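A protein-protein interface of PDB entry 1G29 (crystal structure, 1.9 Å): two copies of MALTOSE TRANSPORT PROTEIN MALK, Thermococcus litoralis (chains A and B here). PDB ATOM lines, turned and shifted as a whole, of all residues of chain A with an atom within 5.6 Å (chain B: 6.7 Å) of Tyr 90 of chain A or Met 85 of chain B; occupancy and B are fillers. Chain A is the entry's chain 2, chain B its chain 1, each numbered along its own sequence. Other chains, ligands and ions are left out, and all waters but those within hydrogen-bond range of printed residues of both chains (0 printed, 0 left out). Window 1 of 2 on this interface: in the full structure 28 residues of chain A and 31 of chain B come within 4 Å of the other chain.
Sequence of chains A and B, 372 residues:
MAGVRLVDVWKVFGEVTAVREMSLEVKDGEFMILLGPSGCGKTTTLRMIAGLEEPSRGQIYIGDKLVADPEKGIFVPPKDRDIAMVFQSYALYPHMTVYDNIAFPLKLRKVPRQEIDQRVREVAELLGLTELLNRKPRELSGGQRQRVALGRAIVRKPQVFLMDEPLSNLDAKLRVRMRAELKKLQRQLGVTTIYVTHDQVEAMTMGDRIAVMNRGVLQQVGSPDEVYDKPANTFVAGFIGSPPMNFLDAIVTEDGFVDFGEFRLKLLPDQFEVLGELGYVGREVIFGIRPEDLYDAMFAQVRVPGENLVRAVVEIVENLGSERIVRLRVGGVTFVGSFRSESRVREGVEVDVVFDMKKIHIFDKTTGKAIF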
ATOM      1  N   LEU A  52     -17.655  -5.324  11.170  1.00  0.00           N
ATOM      2  CA  LEU A  52     -18.410  -5.090  12.402  1.00  0.00           C
ATOM      3  C   LEU A  52     -19.488  -4.015  12.178  1.00  0.00           C
ATOM      4  O   LEU A  52     -20.332  -3.786  13.018  1.00  0.00           O
ATOM      5  CB  LEU A  52     -17.468  -4.612  13.501  1.00  0.00           C
ATOM      6  CG  LEU A  52     -16.437  -5.662  13.913  1.00  0.00           C
ATOM      7  CD1 LEU A  52     -15.359  -4.949  14.729  1.00  0.00           C
ATOM      8  CD2 LEU A  52     -17.143  -6.754  14.772  1.00  0.00           C
ATOM      9  N   MET A  85      -8.846  -9.159  13.657  1.00  0.00           N
ATOM     10  CA  MET A  85      -9.046  -7.923  14.401  1.00  0.00           C
ATOM     11  C   MET A  85      -8.312  -8.288  15.666  1.00  0.00           C
ATOM     12  O   MET A  85      -8.819  -9.102  16.448  1.00  0.00           O
ATOM     13  CB  MET A  85     -10.512  -7.710  14.777  1.00  0.00           C
ATOM     14  CG  MET A  85     -11.530  -7.815  13.672  1.00  0.00           C
ATOM     15  SD  MET A  85     -13.215  -7.864  14.399  1.00  0.00           S
ATOM     16  CE  MET A  85     -13.730  -9.609  14.096  1.00  0.00           C
ATOM     17  N   PHE A  87      -8.224  -7.594  18.545  1.00  0.00           N
ATOM     18  CA  PHE A  87      -9.016  -6.975  19.614  1.00  0.00           C
ATOM     19  C   PHE A  87      -9.614  -8.099  20.455  1.00  0.00           C
ATOM     20  O   PHE A  87     -10.570  -8.774  20.054  1.00  0.00           O
ATOM     21  CB  PHE A  87     -10.126  -6.122  18.999  1.00  0.00           C
ATOM     22  CG  PHE A  87     -10.873  -5.283  19.993  1.00  0.00           C
ATOM     23  CD1 PHE A  87     -12.113  -5.692  20.484  1.00  0.00           C
ATOM     24  CD2 PHE A  87     -10.357  -4.057  20.412  1.00  0.00           C
ATOM     25  CE1 PHE A  87     -12.835  -4.890  21.381  1.00  0.00           C
ATOM     26  CE2 PHE A  87     -11.071  -3.243  21.312  1.00  0.00           C
ATOM     27  CZ  PHE A  87     -12.311  -3.663  21.791  1.00  0.00           C
ATOM     28  N   GLN A  88      -9.039  -8.263  21.633  1.00  0.00           N
ATOM     29  CA  GLN A  88      -9.385  -9.316  22.584  1.00  0.00           C
ATOM     30  C   GLN A  88     -10.844  -9.595  22.927  1.00  0.00           C
ATOM     31  O   GLN A  88     -11.291 -10.740  22.893  1.00  0.00           O
ATOM     32  CB  GLN A  88      -8.588  -9.079  23.879  1.00  0.00           C
ATOM     33  CG  GLN A  88      -8.862 -10.086  24.969  1.00  0.00           C
ATOM     34  CD  GLN A  88      -9.948  -9.626  25.920  1.00  0.00           C
ATOM     35  OE1 GLN A  88      -9.877  -8.521  26.464  1.00  0.00           O
ATOM     36  NE2 GLN A  88     -10.949 -10.469  26.135  1.00  0.00           N
ATOM     37  N   SER A  89     -11.596  -8.564  23.260  1.00  0.00           N
ATOM     38  CA  SER A  89     -12.986  -8.783  23.633  1.00  0.00           C
ATOM     39  C   SER A  89     -13.796  -9.511  22.560  1.00  0.00           C
ATOM     40  O   SER A  89     -14.721 -10.267  22.877  1.00  0.00           O
ATOM     41  CB  SER A  89     -13.636  -7.444  23.983  1.00  0.00           C
ATOM     42  OG  SER A  89     -12.908  -6.807  25.023  1.00  0.00           O
ATOM     43  N   TYR A  90     -13.434  -9.296  21.293  1.00  0.00           N
ATOM     44  CA  TYR A  90     -14.139  -9.920  20.167  1.00  0.00           C
ATOM     45  C   TYR A  90     -13.557 -11.263  19.709  1.00  0.00           C
ATOM     46  O   TYR A  90     -14.280 -12.161  19.300  1.00  0.00           O
ATOM     47  CB  TYR A  90     -14.150  -8.986  18.941  1.00  0.00           C
ATOM     48  CG  TYR A  90     -14.780  -7.612  19.119  1.00  0.00           C
ATOM     49  CD1 TYR A  90     -15.634  -7.321  20.187  1.00  0.00           C
ATOM     50  CD2 TYR A  90     -14.554  -6.610  18.179  1.00  0.00           C
ATOM     51  CE1 TYR A  90     -16.252  -6.046  20.303  1.00  0.00           C
ATOM     52  CE2 TYR A  90     -15.160  -5.350  18.282  1.00  0.00           C
ATOM     53  CZ  TYR A  90     -16.003  -5.067  19.337  1.00  0.00           C
ATOM     54  OH  TYR A  90     -16.579  -3.806  19.416  1.00  0.00           O
ATOM     55  N   ALA A  91     -12.245 -11.404  19.790  1.00  0.00           N
ATOM     56  CA  ALA A  91     -11.591 -12.605  19.300  1.00  0.00           C
ATOM     57  C   ALA A  91     -11.583 -13.824  20.216  1.00  0.00           C
ATOM     58  O   ALA A  91     -11.572 -14.972  19.757  1.00  0.00           O
ATOM     59  CB  ALA A  91     -10.146 -12.246  18.933  1.00  0.00           C
ATOM     60  N   LEU A  92     -11.625 -13.567  21.513  1.00  0.00           N
ATOM     61  CA  LEU A  92     -11.472 -14.618  22.503  1.00  0.00           C
ATOM     62  C   LEU A  92     -12.677 -15.215  23.254  1.00  0.00           C
ATOM     63  O   LEU A  92     -13.622 -14.510  23.565  1.00  0.00           O
ATOM     64  CB  LEU A  92     -10.423 -14.065  23.455  1.00  0.00           C
ATOM     65  CG  LEU A  92     -10.078 -14.327  24.900  1.00  0.00           C
ATOM     66  CD1 LEU A  92      -8.675 -13.647  25.131  1.00  0.00           C
ATOM     67  CD2 LEU A  92     -11.141 -13.732  25.840  1.00  0.00           C
ATOM     68  N   ARG B  47     -22.270 -14.198  21.700  1.00  0.00           N
ATOM     69  CA  ARG B  47     -21.688 -13.667  20.451  1.00  0.00           C
ATOM     70  C   ARG B  47     -22.735 -13.551  19.306  1.00  0.00           C
ATOM     71  O   ARG B  47     -22.669 -12.603  18.504  1.00  0.00           O
ATOM     72  CB  ARG B  47     -20.490 -14.531  20.002  1.00  0.00           C
ATOM     73  CG  ARG B  47     -19.238 -14.301  20.891  1.00  0.00           C
ATOM     74  CD  ARG B  47     -18.187 -15.441  20.721  1.00  0.00           C
ATOM     75  NE  ARG B  47     -17.539 -15.349  19.432  1.00  0.00           N
ATOM     76  CZ  ARG B  47     -16.595 -14.444  19.139  1.00  0.00           C
ATOM     77  NH1 ARG B  47     -16.203 -13.582  20.064  1.00  0.00           N
ATOM     78  NH2 ARG B  47     -16.071 -14.371  17.917  1.00  0.00           N
ATOM     79  N   ALA B  50     -24.818 -10.539  20.017  1.00  0.00           N
ATOM     80  CA  ALA B  50     -24.046  -9.296  19.741  1.00  0.00           C
ATOM     81  C   ALA B  50     -23.874  -9.092  18.227  1.00  0.00           C
ATOM     82  O   ALA B  50     -23.830  -7.957  17.729  1.00  0.00           O
ATOM     83  CB  ALA B  50     -22.671  -9.393  20.385  1.00  0.00           C
ATOM     84  N   GLY B  51     -23.771 -10.201  17.494  1.00  0.00           N
ATOM     85  CA  GLY B  51     -23.570 -10.105  16.061  1.00  0.00           C
ATOM     86  C   GLY B  51     -22.102 -10.363  15.711  1.00  0.00           C
ATOM     87  O   GLY B  51     -21.665 -10.103  14.573  1.00  0.00           O
ATOM     88  N   LEU B  52     -21.305 -10.841  16.663  1.00  0.00           N
ATOM     89  CA  LEU B  52     -19.909 -11.131  16.326  1.00  0.00           C
ATOM     90  C   LEU B  52     -19.912 -12.451  15.517  1.00  0.00           C
ATOM     91  O   LEU B  52     -18.948 -12.745  14.789  1.00  0.00           O
ATOM     92  CB  LEU B  52     -19.092 -11.321  17.600  1.00  0.00           C
ATOM     93  CG  LEU B  52     -18.933 -10.033  18.420  1.00  0.00           C
ATOM     94  CD1 LEU B  52     -18.309 -10.342  19.824  1.00  0.00           C
ATOM     95  CD2 LEU B  52     -18.086  -9.090  17.630  1.00  0.00           C
ATOM     96  N   GLU B  53     -20.974 -13.251  15.672  1.00  0.00           N
ATOM     97  CA  GLU B  53     -21.065 -14.531  14.929  1.00  0.00           C
ATOM     98  C   GLU B  53     -22.462 -14.615  14.348  1.00  0.00           C
ATOM     99  O   GLU B  53     -23.445 -14.281  15.023  1.00  0.00           O
ATOM    100  CB  GLU B  53     -20.914 -15.737  15.868  1.00  0.00           C
ATOM    101  CG  GLU B  53     -19.652 -15.758  16.686  1.00  0.00           C
ATOM    102  CD  GLU B  53     -18.549 -16.593  16.087  1.00  0.00           C
ATOM    103  OE1 GLU B  53     -17.389 -16.380  16.515  1.00  0.00           O
ATOM    104  OE2 GLU B  53     -18.818 -17.456  15.201  1.00  0.00           O
ATOM    105  N   PRO B  78     -22.780  -6.121  14.433  1.00  0.00           N
ATOM    106  CA  PRO B  78     -22.802  -5.566  15.786  1.00  0.00           C
ATOM    107  C   PRO B  78     -23.002  -4.083  15.947  1.00  0.00           C
ATOM    108  O   PRO B  78     -23.869  -3.662  16.695  1.00  0.00           O
ATOM    109  CB  PRO B  78     -21.464  -6.015  16.383  1.00  0.00           C
ATOM    110  CG  PRO B  78     -21.125  -7.220  15.635  1.00  0.00           C
ATOM    111  CD  PRO B  78     -21.546  -6.900  14.204  1.00  0.00           C
ATOM    112  N   LYS B  79     -22.215  -3.289  15.241  1.00  0.00           N
ATOM    113  CA  LYS B  79     -22.334  -1.838  15.420  1.00  0.00           C
ATOM    114  C   LYS B  79     -23.700  -1.322  14.969  1.00  0.00           C
ATOM    115  O   LYS B  79     -24.192  -0.312  15.488  1.00  0.00           O
ATOM    116  CB  LYS B  79     -21.199  -1.102  14.689  1.00  0.00           C
ATOM    117  CG  LYS B  79     -21.219   0.441  14.952  1.00  0.00           C
ATOM    118  CD  LYS B  79     -20.922   0.773  16.442  1.00  0.00           C
ATOM    119  CE  LYS B  79     -21.186   2.275  16.745  1.00  0.00           C
ATOM    120  NZ  LYS B  79     -20.998   2.596  18.229  1.00  0.00           N
ATOM    121  N   ILE B  83     -27.349  -2.569  20.606  1.00  0.00           N
ATOM    122  CA  ILE B  83     -26.761  -3.306  21.702  1.00  0.00           C
ATOM    123  C   ILE B  83     -25.514  -2.585  22.195  1.00  0.00           C
ATOM    124  O   ILE B  83     -24.915  -1.772  21.472  1.00  0.00           O
ATOM    125  CB  ILE B  83     -26.329  -4.712  21.228  1.00  0.00           C
ATOM    126  CG1 ILE B  83     -25.349  -4.569  20.056  1.00  0.00           C
ATOM    127  CG2 ILE B  83     -27.541  -5.481  20.690  1.00  0.00           C
ATOM    128  CD1 ILE B  83     -24.023  -5.346  20.196  1.00  0.00           C
ATOM    129  N   ALA B  84     -25.153  -2.857  23.447  1.00  0.00           N
ATOM    130  CA  ALA B  84     -23.939  -2.297  24.038  1.00  0.00           C
ATOM    131  C   ALA B  84     -23.183  -3.504  24.588  1.00  0.00           C
ATOM    132  O   ALA B  84     -23.715  -4.198  25.438  1.00  0.00           O
ATOM    133  CB  ALA B  84     -24.283  -1.366  25.177  1.00  0.00           C
ATOM    134  N   MET B  85     -21.985  -3.755  24.075  1.00  0.00           N
ATOM    135  CA  MET B  85     -21.159  -4.843  24.567  1.00  0.00           C
ATOM    136  C   MET B  85     -20.294  -4.196  25.639  1.00  0.00           C
ATOM    137  O   MET B  85     -19.643  -3.186  25.389  1.00  0.00           O
ATOM    138  CB  MET B  85     -20.266  -5.395  23.448  1.00  0.00           C
ATOM    139  CG  MET B  85     -21.037  -6.242  22.397  1.00  0.00           C
ATOM    140  SD  MET B  85     -19.898  -6.904  21.098  1.00  0.00           S
ATOM    141  CE  MET B  85     -20.173  -5.817  19.932  1.00  0.00           C
ATOM    142  N   VAL B  86     -20.267  -4.793  26.815  1.00  0.00           N
ATOM    143  CA  VAL B  86     -19.486  -4.248  27.916  1.00  0.00           C
ATOM    144  C   VAL B  86     -18.296  -5.154  28.098  1.00  0.00           C
ATOM    145  O   VAL B  86     -18.481  -6.349  28.347  1.00  0.00           O
ATOM    146  CB  VAL B  86     -20.325  -4.242  29.212  1.00  0.00           C
ATOM    147  CG1 VAL B  86     -19.577  -3.546  30.347  1.00  0.00           C
ATOM    148  CG2 VAL B  86     -21.625  -3.576  28.950  1.00  0.00           C
ATOM    149  N   PHE B  87     -17.080  -4.622  27.936  1.00  0.00           N
ATOM    150  CA  PHE B  87     -15.880  -5.448  28.125  1.00  0.00           C
ATOM    151  C   PHE B  87     -14.740  -4.715  28.870  1.00  0.00           C
ATOM    152  O   PHE B  87     -14.999  -3.981  29.826  1.00  0.00           O
ATOM    153  CB  PHE B  87     -15.385  -6.014  26.776  1.00  0.00           C
ATOM    154  CG  PHE B  87     -16.205  -7.208  26.255  1.00  0.00           C
ATOM    155  CD1 PHE B  87     -17.428  -7.020  25.595  1.00  0.00           C
ATOM    156  CD2 PHE B  87     -15.755  -8.521  26.427  1.00  0.00           C
ATOM    157  CE1 PHE B  87     -18.194  -8.123  25.112  1.00  0.00           C
ATOM    158  CE2 PHE B  87     -16.518  -9.627  25.944  1.00  0.00           C
ATOM    159  CZ  PHE B  87     -17.740  -9.416  25.288  1.00  0.00           C
ATOM    160  N   TYR B  90     -13.088   0.575  26.985  1.00  0.00           N
ATOM    161  CA  TYR B  90     -13.200   1.049  25.615  1.00  0.00           C
ATOM    162  C   TYR B  90     -12.575   2.379  25.203  1.00  0.00           C
ATOM    163  O   TYR B  90     -11.857   3.023  25.980  1.00  0.00           O
ATOM    164  CB  TYR B  90     -14.669   0.961  25.163  1.00  0.00           C
ATOM    165  CG  TYR B  90     -15.095  -0.484  24.927  1.00  0.00           C
ATOM    166  CD1 TYR B  90     -15.659  -1.256  25.954  1.00  0.00           C
ATOM    167  CD2 TYR B  90     -14.847  -1.112  23.697  1.00  0.00           C
ATOM    168  CE1 TYR B  90     -15.959  -2.627  25.760  1.00  0.00           C
ATOM    169  CE2 TYR B  90     -15.144  -2.477  23.495  1.00  0.00           C
ATOM    170  CZ  TYR B  90     -15.697  -3.228  24.528  1.00  0.00           C
ATOM    171  OH  TYR B  90     -15.986  -4.563  24.331  1.00  0.00           O
ATOM    172  N   ALA B 153     -21.545   4.417  26.996  1.00  0.00           N
ATOM    173  CA  ALA B 153     -22.449   3.367  26.497  1.00  0.00           C
ATOM    174  C   ALA B 153     -23.879   3.542  27.032  1.00  0.00           C
ATOM    175  O   ALA B 153     -24.858   3.425  26.282  1.00  0.00           O
ATOM    176  CB  ALA B 153     -21.915   2.011  26.902  1.00  0.00           C
ATOM    177  N   VAL B 160     -30.143  -3.448  24.815  1.00  0.00           N
ATOM    178  CA  VAL B 160     -29.607  -4.482  25.717  1.00  0.00           C
ATOM    179  C   VAL B 160     -28.114  -4.328  25.911  1.00  0.00           C
ATOM    180  O   VAL B 160     -27.383  -3.879  25.000  1.00  0.00           O
ATOM    181  CB  VAL B 160     -29.953  -5.939  25.159  1.00  0.00           C
ATOM    182  CG1 VAL B 160     -29.313  -6.162  23.764  1.00  0.00           C
ATOM    183  CG2 VAL B 160     -29.414  -7.095  26.115  1.00  0.00           C
ATOM    184  N   PHE B 161     -27.661  -4.672  27.121  1.00  0.00           N
ATOM    185  CA  PHE B 161     -26.241  -4.661  27.453  1.00  0.00           C
ATOM    186  C   PHE B 161     -25.815  -6.103  27.467  1.00  0.00           C
ATOM    187  O   PHE B 161     -26.515  -6.917  28.064  1.00  0.00           O
ATOM    188  CB  PHE B 161     -25.990  -4.123  28.856  1.00  0.00           C
ATOM    189  CG  PHE B 161     -26.029  -2.616  28.918  1.00  0.00           C
ATOM    190  CD1 PHE B 161     -24.923  -1.884  28.627  1.00  0.00           C
ATOM    191  CD2 PHE B 161     -27.214  -1.971  29.215  1.00  0.00           C
ATOM    192  CE1 PHE B 161     -24.981  -0.454  28.629  1.00  0.00           C
ATOM    193  CE2 PHE B 161     -27.284  -0.557  29.218  1.00  0.00           C
ATOM    194  CZ  PHE B 161     -26.169   0.171  28.926  1.00  0.00           C
ATOM    195  N   LEU B 162     -24.642  -6.387  26.892  1.00  0.00           N
ATOM    196  CA  LEU B 162     -24.140  -7.777  26.826  1.00  0.00           C
ATOM    197  C   LEU B 162     -22.772  -7.846  27.504  1.00  0.00           C
ATOM    198  O   LEU B 162     -21.887  -7.009  27.229  1.00  0.00           O
ATOM    199  CB  LEU B 162     -23.985  -8.173  25.350  1.00  0.00           C
ATOM    200  CG  LEU B 162     -25.253  -7.985  24.494  1.00  0.00           C
ATOM    201  CD1 LEU B 162     -24.870  -8.382  23.030  1.00  0.00           C
ATOM    202  CD2 LEU B 162     -26.397  -8.923  25.041  1.00  0.00           C
ATOM    203  N   MET B 163     -22.579  -8.812  28.407  1.00  0.00           N
ATOM    204  CA  MET B 163     -21.271  -8.932  29.012  1.00  0.00           C
ATOM    205  C   MET B 163     -20.942 -10.389  29.303  1.00  0.00           C
ATOM    206  O   MET B 163     -21.856 -11.187  29.547  1.00  0.00           O
ATOM    207  CB  MET B 163     -21.194  -8.089  30.303  1.00  0.00           C
ATOM    208  CG  MET B 163     -22.299  -8.280  31.259  1.00  0.00           C
ATOM    209  SD  MET B 163     -22.419  -6.703  32.308  1.00  0.00           S
ATOM    210  CE  MET B 163     -23.780  -5.748  31.340  1.00  0.00           C
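Hydrophobic or aromatic side chains of chain A that line the printed part of chain B: Leu 52, Phe 87 and Tyr 90.
Of the 18 printed residues of chain B, 7 touch a printed residue of chain A.
Among the printed residues, 9 pairs touch across the chains.
Printed residues of chain B within 4 Å of Phe 87 of chain A: Tyr 90 (3.5 Å).
Of chain B, only Arg 47, Leu 52 and Met 85 come within 4 Å of Tyr 90 of chain A.
Gly 51 of chain B touches none of the printed residues of chain A.
Printed residues of chain A within 4 Å of Pro 78 of chain B: Leu 52 (3.5 Å).
Of chain A, only Tyr 90 (3.8 Å) comes within 4 Å of Met 85 of chain B.
Val 86 of chain B touches none of the printed residues of chain A.
Of the printed residues of chain A, Phe 87 of chain B touches Ser 89.
Of the printed residues of chain A, Tyr 90 of chain B touches Phe 87 (3.5 Å) and Ser 89 (3.7 Å).
The nearest printed residue of chain A that does not touch Met 85 of chain B is Leu 52 of chain A (6.1 Å).
The nearest printed residue of chain A that does not touch Arg 47 of chain B is Leu 92 of chain A (4.4 Å).
Leu 52 of chain B touches its own counterpart, Leu 52 of chain A.
Phe 87 of chain A touches Tyr 90 of chain B, but with the chains exchanged Tyr 90 of chain A does not touch Phe 87 of chain B (5.5 Å).
Tyr 90 of chain A touches Leu 52 of chain B, but with the chains exchanged Leu 52 of chain A does not touch Tyr 90 of chain B (9.1 Å).
Tyr 90 of chain A touches Met 85 of chain B, but with the chains exchanged Met 85 of chain A does not touch Tyr 90 of chain B (10.7 Å).
Positions printed for both chains: 52, 85, 87 and 90.
Of the 9 pairs that touch across the chains among the printed residues, 1 has its exchanged pair printed and touching as well.
The guanidinium group (NH1) of Arg 47 of chain B is in hydrogen-bond range of the backbone carbonyl oxygen (O) of Tyr 90 of chain A (2.5 Å).
The backbone NH (N) of Lys 79 of chain B lies within hydrogen-bond range of the backbone carbonyl oxygen (O) of Leu 52 of chain A, 3.0 Å away.
CD2 of Leu 52 of chain B touches CD2 of Leu 52 of chain A, at 3.8 Å.
Pro 78 of chain B touches Leu 52 of chain A (CD to O, 3.5 Å).
CZ of Phe 87 of chain A touches CE2 of Tyr 90 of chain B (3.5 Å).
Ser 89 of chain A touches Phe 87 of chain B.
Tyr 90 of chain B touches Ser 89 of chain A.
CG of Tyr 90 of chain A touches CD2 of Leu 52 of chain B, at 3.9 Å.
Tyr 90 of chain A touches Met 85 of chain B.
The backbone carbonyl oxygen (O) of Arg 47 of chain B lies within hydrogen-bond range of the backbone NH (N) of Leu 52 of chain B, at 2.9 Å.
The guanidinium group (NH2) of Arg 47 of chain B is in salt-bridge range of the side-chain carboxylate (OE1) of Glu 53 of chain B, at 2.8 Å.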
